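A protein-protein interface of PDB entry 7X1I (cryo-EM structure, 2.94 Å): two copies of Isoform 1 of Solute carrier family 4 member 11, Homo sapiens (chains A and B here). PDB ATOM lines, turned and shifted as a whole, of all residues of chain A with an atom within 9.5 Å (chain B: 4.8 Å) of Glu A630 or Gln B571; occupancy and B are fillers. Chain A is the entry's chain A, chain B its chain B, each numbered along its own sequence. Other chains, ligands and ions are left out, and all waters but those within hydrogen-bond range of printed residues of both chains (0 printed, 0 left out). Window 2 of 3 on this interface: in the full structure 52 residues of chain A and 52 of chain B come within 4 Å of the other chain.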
ATOM      1  N   GLY A 570      -0.475 -25.134  10.481  1.00  0.00           N
ATOM      2  CA  GLY A 570       0.220 -24.220   9.592  1.00  0.00           C
ATOM      3  C   GLY A 570      -0.379 -22.826   9.593  1.00  0.00           C
ATOM      4  O   GLY A 570       0.132 -21.928  10.258  1.00  0.00           O
ATOM      5  N   GLN A 571      -1.473 -22.650   8.850  1.00  0.00           N
ATOM      6  CA  GLN A 571      -2.136 -21.354   8.777  1.00  0.00           C
ATOM      7  C   GLN A 571      -2.916 -21.016  10.043  1.00  0.00           C
ATOM      8  O   GLN A 571      -3.115 -19.831  10.331  1.00  0.00           O
ATOM      9  CB  GLN A 571      -3.075 -21.312   7.568  1.00  0.00           C
ATOM     10  CG  GLN A 571      -2.373 -21.491   6.229  1.00  0.00           C
ATOM     11  CD  GLN A 571      -3.343 -21.492   5.065  1.00  0.00           C
ATOM     12  OE1 GLN A 571      -4.556 -21.498   5.258  1.00  0.00           O
ATOM     13  NE2 GLN A 571      -2.810 -21.479   3.848  1.00  0.00           N
ATOM     14  N   ALA A 572      -3.361 -22.023  10.799  1.00  0.00           N
ATOM     15  CA  ALA A 572      -4.042 -21.754  12.059  1.00  0.00           C
ATOM     16  C   ALA A 572      -3.103 -21.093  13.064  1.00  0.00           C
ATOM     17  O   ALA A 572      -3.519 -20.213  13.825  1.00  0.00           O
ATOM     18  CB  ALA A 572      -4.628 -23.047  12.628  1.00  0.00           C
ATOM     19  N   THR A 573      -1.833 -21.504  13.077  1.00  0.00           N
ATOM     20  CA  THR A 573      -0.857 -20.880  13.964  1.00  0.00           C
ATOM     21  C   THR A 573      -0.660 -19.405  13.624  1.00  0.00           C
ATOM     22  O   THR A 573      -0.593 -18.556  14.521  1.00  0.00           O
ATOM     23  CB  THR A 573       0.470 -21.635  13.883  1.00  0.00           C
ATOM     24  OG1 THR A 573       0.315 -22.940  14.456  1.00  0.00           O
ATOM     25  CG2 THR A 573       1.570 -20.883  14.619  1.00  0.00           C
ATOM     26  N   ALA A 574      -0.566 -19.082  12.332  1.00  0.00           N
ATOM     27  CA  ALA A 574      -0.339 -17.700  11.918  1.00  0.00           C
ATOM     28  C   ALA A 574      -1.525 -16.812  12.269  1.00  0.00           C
ATOM     29  O   ALA A 574      -1.353 -15.720  12.823  1.00  0.00           O
ATOM     30  CB  ALA A 574      -0.048 -17.650  10.419  1.00  0.00           C
ATOM     31  N   VAL A 575      -2.741 -17.265  11.958  1.00  0.00           N
ATOM     32  CA  VAL A 575      -3.927 -16.463  12.237  1.00  0.00           C
ATOM     33  C   VAL A 575      -4.130 -16.306  13.738  1.00  0.00           C
ATOM     34  O   VAL A 575      -4.444 -15.213  14.223  1.00  0.00           O
ATOM     35  CB  VAL A 575      -5.162 -17.082  11.556  1.00  0.00           C
ATOM     36  CG1 VAL A 575      -6.411 -16.275  11.885  1.00  0.00           C
ATOM     37  CG2 VAL A 575      -4.952 -17.156  10.053  1.00  0.00           C
ATOM     38  N   LEU A 576      -3.952 -17.390  14.499  1.00  0.00           N
ATOM     39  CA  LEU A 576      -4.089 -17.307  15.949  1.00  0.00           C
ATOM     40  C   LEU A 576      -3.032 -16.388  16.548  1.00  0.00           C
ATOM     41  O   LEU A 576      -3.292 -15.692  17.537  1.00  0.00           O
ATOM     42  CB  LEU A 576      -4.003 -18.703  16.568  1.00  0.00           C
ATOM     43  CG  LEU A 576      -4.208 -18.789  18.081  1.00  0.00           C
ATOM     44  CD1 LEU A 576      -5.536 -18.166  18.484  1.00  0.00           C
ATOM     45  CD2 LEU A 576      -4.131 -20.230  18.549  1.00  0.00           C
ATOM     46  N   LEU A 579      -4.362 -13.011  16.285  1.00  0.00           N
ATOM     47  CA  LEU A 579      -5.451 -12.831  17.241  1.00  0.00           C
ATOM     48  C   LEU A 579      -4.927 -12.672  18.663  1.00  0.00           C
ATOM     49  O   LEU A 579      -5.424 -11.831  19.422  1.00  0.00           O
ATOM     50  CB  LEU A 579      -6.420 -14.011  17.158  1.00  0.00           C
ATOM     51  CG  LEU A 579      -7.629 -13.981  18.096  1.00  0.00           C
ATOM     52  CD1 LEU A 579      -8.543 -12.811  17.761  1.00  0.00           C
ATOM     53  CD2 LEU A 579      -8.392 -15.297  18.034  1.00  0.00           C
ATOM     54  N   ILE A 623      -5.564 -18.779  27.155  1.00  0.00           N
ATOM     55  CA  ILE A 623      -6.356 -18.889  25.931  1.00  0.00           C
ATOM     56  C   ILE A 623      -5.551 -19.579  24.837  1.00  0.00           C
ATOM     57  O   ILE A 623      -6.049 -20.472  24.141  1.00  0.00           O
ATOM     58  CB  ILE A 623      -6.846 -17.500  25.482  1.00  0.00           C
ATOM     59  CG1 ILE A 623      -7.829 -16.926  26.502  1.00  0.00           C
ATOM     60  CG2 ILE A 623      -7.490 -17.579  24.105  1.00  0.00           C
ATOM     61  CD1 ILE A 623      -8.327 -15.540  26.159  1.00  0.00           C
ATOM     62  N   SER A 624      -4.288 -19.183  24.676  1.00  0.00           N
ATOM     63  CA  SER A 624      -3.467 -19.747  23.611  1.00  0.00           C
ATOM     64  C   SER A 624      -3.028 -21.173  23.921  1.00  0.00           C
ATOM     65  O   SER A 624      -3.037 -22.032  23.033  1.00  0.00           O
ATOM     66  CB  SER A 624      -2.249 -18.855  23.366  1.00  0.00           C
ATOM     67  OG  SER A 624      -1.446 -19.367  22.316  1.00  0.00           O
ATOM     68  N   SER A 625      -2.649 -21.448  25.171  1.00  0.00           N
ATOM     69  CA  SER A 625      -2.100 -22.750  25.525  1.00  0.00           C
ATOM     70  C   SER A 625      -3.154 -23.758  25.966  1.00  0.00           C
ATOM     71  O   SER A 625      -2.918 -24.965  25.844  1.00  0.00           O
ATOM     72  CB  SER A 625      -1.055 -22.600  26.635  1.00  0.00           C
ATOM     73  OG  SER A 625       0.008 -21.757  26.227  1.00  0.00           O
ATOM     74  N   HIS A 626      -4.298 -23.306  26.469  1.00  0.00           N
ATOM     75  CA  HIS A 626      -5.345 -24.216  26.929  1.00  0.00           C
ATOM     76  C   HIS A 626      -6.623 -24.123  26.114  1.00  0.00           C
ATOM     77  O   HIS A 626      -7.268 -25.145  25.873  1.00  0.00           O
ATOM     78  CB  HIS A 626      -5.665 -23.956  28.410  1.00  0.00           C
ATOM     79  CG  HIS A 626      -6.706 -24.875  28.972  1.00  0.00           C
ATOM     80  ND1 HIS A 626      -6.530 -26.239  29.048  1.00  0.00           N
ATOM     81  CD2 HIS A 626      -7.935 -24.625  29.482  1.00  0.00           C
ATOM     82  CE1 HIS A 626      -7.605 -26.791  29.582  1.00  0.00           C
ATOM     83  NE2 HIS A 626      -8.473 -25.834  29.854  1.00  0.00           N
ATOM     84  N   GLY A 627      -7.015 -22.920  25.685  1.00  0.00           N
ATOM     85  CA  GLY A 627      -8.179 -22.783  24.828  1.00  0.00           C
ATOM     86  C   GLY A 627      -7.943 -23.212  23.395  1.00  0.00           C
ATOM     87  O   GLY A 627      -8.908 -23.509  22.682  1.00  0.00           O
ATOM     88  N   PHE A 628      -6.687 -23.244  22.959  1.00  0.00           N
ATOM     89  CA  PHE A 628      -6.306 -23.624  21.601  1.00  0.00           C
ATOM     90  C   PHE A 628      -5.175 -24.645  21.632  1.00  0.00           C
ATOM     91  O   PHE A 628      -4.153 -24.501  20.957  1.00  0.00           O
ATOM     92  CB  PHE A 628      -5.904 -22.401  20.779  1.00  0.00           C
ATOM     93  CG  PHE A 628      -7.036 -21.448  20.512  1.00  0.00           C
ATOM     94  CD1 PHE A 628      -7.976 -21.723  19.532  1.00  0.00           C
ATOM     95  CD2 PHE A 628      -7.153 -20.271  21.234  1.00  0.00           C
ATOM     96  CE1 PHE A 628      -9.016 -20.847  19.283  1.00  0.00           C
ATOM     97  CE2 PHE A 628      -8.190 -19.391  20.990  1.00  0.00           C
ATOM     98  CZ  PHE A 628      -9.122 -19.680  20.012  1.00  0.00           C
ATOM     99  N   ARG A 629      -5.344 -25.691  22.445  1.00  0.00           N
ATOM    100  CA  ARG A 629      -4.320 -26.729  22.543  1.00  0.00           C
ATOM    101  C   ARG A 629      -4.053 -27.394  21.198  1.00  0.00           C
ATOM    102  O   ARG A 629      -2.909 -27.768  20.908  1.00  0.00           O
ATOM    103  CB  ARG A 629      -4.736 -27.787  23.566  1.00  0.00           C
ATOM    104  CG  ARG A 629      -5.021 -27.245  24.954  1.00  0.00           C
ATOM    105  CD  ARG A 629      -5.477 -28.355  25.885  1.00  0.00           C
ATOM    106  NE  ARG A 629      -6.599 -29.100  25.325  1.00  0.00           N
ATOM    107  CZ  ARG A 629      -7.872 -28.754  25.467  1.00  0.00           C
ATOM    108  NH1 ARG A 629      -8.224 -27.673  26.143  1.00  0.00           N
ATOM    109  NH2 ARG A 629      -8.815 -29.512  24.916  1.00  0.00           N
ATOM    110  N   GLU A 630      -5.084 -27.541  20.364  1.00  0.00           N
ATOM    111  CA  GLU A 630      -4.938 -28.227  19.085  1.00  0.00           C
ATOM    112  C   GLU A 630      -4.120 -27.434  18.073  1.00  0.00           C
ATOM    113  O   GLU A 630      -3.749 -27.993  17.035  1.00  0.00           O
ATOM    114  CB  GLU A 630      -6.318 -28.542  18.498  1.00  0.00           C
ATOM    115  CG  GLU A 630      -7.222 -29.379  19.402  1.00  0.00           C
ATOM    116  CD  GLU A 630      -7.953 -28.547  20.442  1.00  0.00           C
ATOM    117  OE1 GLU A 630      -7.812 -27.306  20.421  1.00  0.00           O
ATOM    118  OE2 GLU A 630      -8.667 -29.134  21.281  1.00  0.00           O
ATOM    119  N   ILE A 631      -3.829 -26.164  18.344  1.00  0.00           N
ATOM    120  CA  ILE A 631      -3.104 -25.296  17.423  1.00  0.00           C
ATOM    121  C   ILE A 631      -1.700 -25.088  17.972  1.00  0.00           C
ATOM    122  O   ILE A 631      -1.530 -24.630  19.110  1.00  0.00           O
ATOM    123  CB  ILE A 631      -3.823 -23.952  17.224  1.00  0.00           C
ATOM    124  CG1 ILE A 631      -5.226 -24.175  16.652  1.00  0.00           C
ATOM    125  CG2 ILE A 631      -3.014 -23.046  16.310  1.00  0.00           C
ATOM    126  CD1 ILE A 631      -6.009 -22.896  16.440  1.00  0.00           C
ATOM    127  N   GLU A 632      -0.696 -25.430  17.169  1.00  0.00           N
ATOM    128  CA  GLU A 632       0.686 -25.166  17.545  1.00  0.00           C
ATOM    129  C   GLU A 632       0.934 -23.665  17.616  1.00  0.00           C
ATOM    130  O   GLU A 632       0.396 -22.889  16.822  1.00  0.00           O
ATOM    131  CB  GLU A 632       1.642 -25.812  16.539  1.00  0.00           C
ATOM    132  CG  GLU A 632       3.119 -25.575  16.830  1.00  0.00           C
ATOM    133  CD  GLU A 632       4.005 -25.890  15.640  1.00  0.00           C
ATOM    134  OE1 GLU A 632       3.464 -26.262  14.576  1.00  0.00           O
ATOM    135  OE2 GLU A 632       5.240 -25.764  15.766  1.00  0.00           O
ATOM    136  N   MET A 633       1.742 -23.254  18.588  1.00  0.00           N
ATOM    137  CA  MET A 633       2.117 -21.859  18.748  1.00  0.00           C
ATOM    138  C   MET A 633       3.633 -21.728  18.766  1.00  0.00           C
ATOM    139  O   MET A 633       4.344 -22.602  19.275  1.00  0.00           O
ATOM    140  CB  MET A 633       1.516 -21.263  20.029  1.00  0.00           C
ATOM    141  CG  MET A 633       0.002 -21.119  19.992  1.00  0.00           C
ATOM    142  SD  MET A 633      -0.554 -19.969  18.720  1.00  0.00           S
ATOM    143  CE  MET A 633       0.190 -18.446  19.297  1.00  0.00           C
ATOM    144  N   TYR B 517     -15.811 -26.569  11.770  1.00  0.00           N
ATOM    145  CA  TYR B 517     -14.474 -26.439  11.201  1.00  0.00           C
ATOM    146  C   TYR B 517     -13.362 -26.795  12.180  1.00  0.00           C
ATOM    147  O   TYR B 517     -12.494 -27.611  11.853  1.00  0.00           O
ATOM    148  CB  TYR B 517     -14.266 -25.014  10.674  1.00  0.00           C
ATOM    149  CG  TYR B 517     -15.108 -24.679   9.463  1.00  0.00           C
ATOM    150  CD1 TYR B 517     -14.691 -25.032   8.185  1.00  0.00           C
ATOM    151  CD2 TYR B 517     -16.316 -24.008   9.595  1.00  0.00           C
ATOM    152  CE1 TYR B 517     -15.454 -24.729   7.076  1.00  0.00           C
ATOM    153  CE2 TYR B 517     -17.087 -23.699   8.490  1.00  0.00           C
ATOM    154  CZ  TYR B 517     -16.651 -24.062   7.233  1.00  0.00           C
ATOM    155  OH  TYR B 517     -17.414 -23.757   6.130  1.00  0.00           O
ATOM    156  N   TYR B 518     -13.364 -26.195  13.374  1.00  0.00           N
ATOM    157  CA  TYR B 518     -12.274 -26.417  14.321  1.00  0.00           C
ATOM    158  C   TYR B 518     -12.195 -27.880  14.740  1.00  0.00           C
ATOM    159  O   TYR B 518     -11.104 -28.459  14.815  1.00  0.00           O
ATOM    160  CB  TYR B 518     -12.448 -25.512  15.543  1.00  0.00           C
ATOM    161  CG  TYR B 518     -11.235 -25.446  16.445  1.00  0.00           C
ATOM    162  CD1 TYR B 518     -10.240 -24.501  16.233  1.00  0.00           C
ATOM    163  CD2 TYR B 518     -11.087 -26.325  17.511  1.00  0.00           C
ATOM    164  CE1 TYR B 518      -9.130 -24.434  17.055  1.00  0.00           C
ATOM    165  CE2 TYR B 518      -9.981 -26.265  18.338  1.00  0.00           C
ATOM    166  CZ  TYR B 518      -9.006 -25.318  18.105  1.00  0.00           C
ATOM    167  OH  TYR B 518      -7.904 -25.255  18.927  1.00  0.00           O
ATOM    168  N   TYR B 519     -13.340 -28.497  15.022  1.00  0.00           N
ATOM    169  CA  TYR B 519     -13.392 -29.892  15.431  1.00  0.00           C
ATOM    170  C   TYR B 519     -13.724 -30.838  14.285  1.00  0.00           C
ATOM    171  O   TYR B 519     -13.835 -32.047  14.510  1.00  0.00           O
ATOM    172  CB  TYR B 519     -14.402 -30.072  16.570  1.00  0.00           C
ATOM    173  CG  TYR B 519     -14.078 -29.240  17.791  1.00  0.00           C
ATOM    174  CD1 TYR B 519     -13.149 -29.678  18.727  1.00  0.00           C
ATOM    175  CD2 TYR B 519     -14.693 -28.014  18.004  1.00  0.00           C
ATOM    176  CE1 TYR B 519     -12.845 -28.918  19.842  1.00  0.00           C
ATOM    177  CE2 TYR B 519     -14.397 -27.247  19.116  1.00  0.00           C
ATOM    178  CZ  TYR B 519     -13.471 -27.704  20.032  1.00  0.00           C
ATOM    179  OH  TYR B 519     -13.174 -26.946  21.140  1.00  0.00           O
ATOM    180  N   GLY B 570      -9.217 -26.014   7.942  1.00  0.00           N
ATOM    181  CA  GLY B 570     -10.018 -26.503   9.049  1.00  0.00           C
ATOM    182  C   GLY B 570     -10.001 -25.571  10.247  1.00  0.00           C
ATOM    183  O   GLY B 570     -10.931 -24.793  10.446  1.00  0.00           O
ATOM    184  N   GLN B 571      -8.932 -25.646  11.042  1.00  0.00           N
ATOM    185  CA  GLN B 571      -8.806 -24.797  12.220  1.00  0.00           C
ATOM    186  C   GLN B 571      -8.473 -23.350  11.873  1.00  0.00           C
ATOM    187  O   GLN B 571      -8.795 -22.452  12.658  1.00  0.00           O
ATOM    188  CB  GLN B 571      -7.737 -25.360  13.161  1.00  0.00           C
ATOM    189  CG  GLN B 571      -8.045 -26.754  13.688  1.00  0.00           C
ATOM    190  CD  GLN B 571      -6.941 -27.292  14.576  1.00  0.00           C
ATOM    191  OE1 GLN B 571      -5.877 -26.688  14.691  1.00  0.00           O
ATOM    192  NE2 GLN B 571      -7.191 -28.431  15.213  1.00  0.00           N
ATOM    193  N   ALA B 572      -7.837 -23.105  10.725  1.00  0.00           N
ATOM    194  CA  ALA B 572      -7.567 -21.734  10.309  1.00  0.00           C
ATOM    195  C   ALA B 572      -8.862 -20.975  10.037  1.00  0.00           C
ATOM    196  O   ALA B 572      -8.965 -19.782  10.344  1.00  0.00           O
ATOM    197  CB  ALA B 572      -6.660 -21.727   9.078  1.00  0.00           C
ATOM    198  N   THR B 573      -9.860 -21.652   9.464  1.00  0.00           N
ATOM    199  CA  THR B 573     -11.152 -21.016   9.226  1.00  0.00           C
ATOM    200  C   THR B 573     -11.820 -20.607  10.536  1.00  0.00           C
ATOM    201  O   THR B 573     -12.375 -19.507  10.643  1.00  0.00           O
ATOM    202  CB  THR B 573     -12.053 -21.961   8.431  1.00  0.00           C
ATOM    203  OG1 THR B 573     -11.532 -22.119   7.104  1.00  0.00           O
ATOM    204  CG2 THR B 573     -13.476 -21.424   8.359  1.00  0.00           C
ATOM    205  N   ALA B 574     -11.775 -21.482  11.544  1.00  0.00           N
ATOM    206  CA  ALA B 574     -12.421 -21.190  12.821  1.00  0.00           C
ATOM    207  C   ALA B 574     -11.751 -20.020  13.529  1.00  0.00           C
ATOM    208  O   ALA B 574     -12.426 -19.103  14.010  1.00  0.00           O
ATOM    209  CB  ALA B 574     -12.413 -22.438  13.703  1.00  0.00           C
ATOM    210  N   VAL B 575     -10.419 -20.033  13.600  1.00  0.00           N
ATOM    211  CA  VAL B 575      -9.701 -18.964  14.285  1.00  0.00           C
ATOM    212  C   VAL B 575      -9.868 -17.644  13.545  1.00  0.00           C
ATOM    213  O   VAL B 575     -10.089 -16.595  14.163  1.00  0.00           O
ATOM    214  CB  VAL B 575      -8.217 -19.339  14.453  1.00  0.00           C
ATOM    215  CG1 VAL B 575      -7.454 -18.205  15.125  1.00  0.00           C
ATOM    216  CG2 VAL B 575      -8.086 -20.622  15.258  1.00  0.00           C
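CB of Ala B572 touches CB of Gln A571, at 3.9 Å. Gln B571 touches Ala A572. N of Ala B572 touches CB of Ala A572 (3.7 Å). CG1 of Val A575 touches CG1 of Val B575, at 3.9 Å. CG1 of Val B575 touches CA of Leu A576 (3.6 Å). Phe A628 touches Tyr B518 (CA to OH, 3.5 Å). Tyr B518 touches Ile A631. OE1 of Gln B571 touches CG1 of Ile A631 (3.3 Å). Ile A631 touches Val B575.
Gly A570 touches none of the printed residues of chain B. Of the printed residues of chain B, Ala A572 touches Gln B571 and Ala B572. His A626 touches none of the printed residues of chain B. Printed residues of chain B within 4 Å of Phe A628: Tyr B518 (3.5 Å). No residue of chain A comes within 4 Å of Gly B570. Gln B571 touches three residues of chain A. No residue of chain A comes within 4 Å of Ala B574.
OE1 of Glu A630 is in hydrogen-bond range of OH of Tyr B518 (2.5 Å). The backbone carbonyl oxygen (O) of Glu A630 sits close to the side-chain amide oxygen (OE1) of Gln B571 (3.4 Å).
The backbone NH of Phe A628 lies within hydrogen-bond range of the backbone carbonyl oxygen of Ile A623 (3.1 Å). The guanidinium group of Arg A629 lies within salt-bridge range of the side-chain carboxylate of Glu A630.
Gln A571 touches Ala B572, and with the chains exchanged Ala A572 touches Gln B571. Ala A572 touches its own counterpart, Ala B572. Val B575 touches its own counterpart, Val A575. Positions printed for both chains: 570, 571, 572, 573, 574 and 575.
Printed residues of chain B that touch a printed residue of chain A: Tyr B518, Gln B571, Ala B572 and Val B575. Along chain B the printed residues that touch a printed residue of chain A span positions 518 to 575. Of the 19 printed residues of chain A, 7 touch a printed residue of chain B. Hydrophobic or aromatic side chains of chain A within 4 Å of the printed part of chain B: Ala A572, Val A575, Leu A576, Phe A628 and Ile A631. Among the printed residues, no Asp or Glu carboxylate lies within 4 Å of a Lys or Arg side-chain nitrogen of the other chain.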
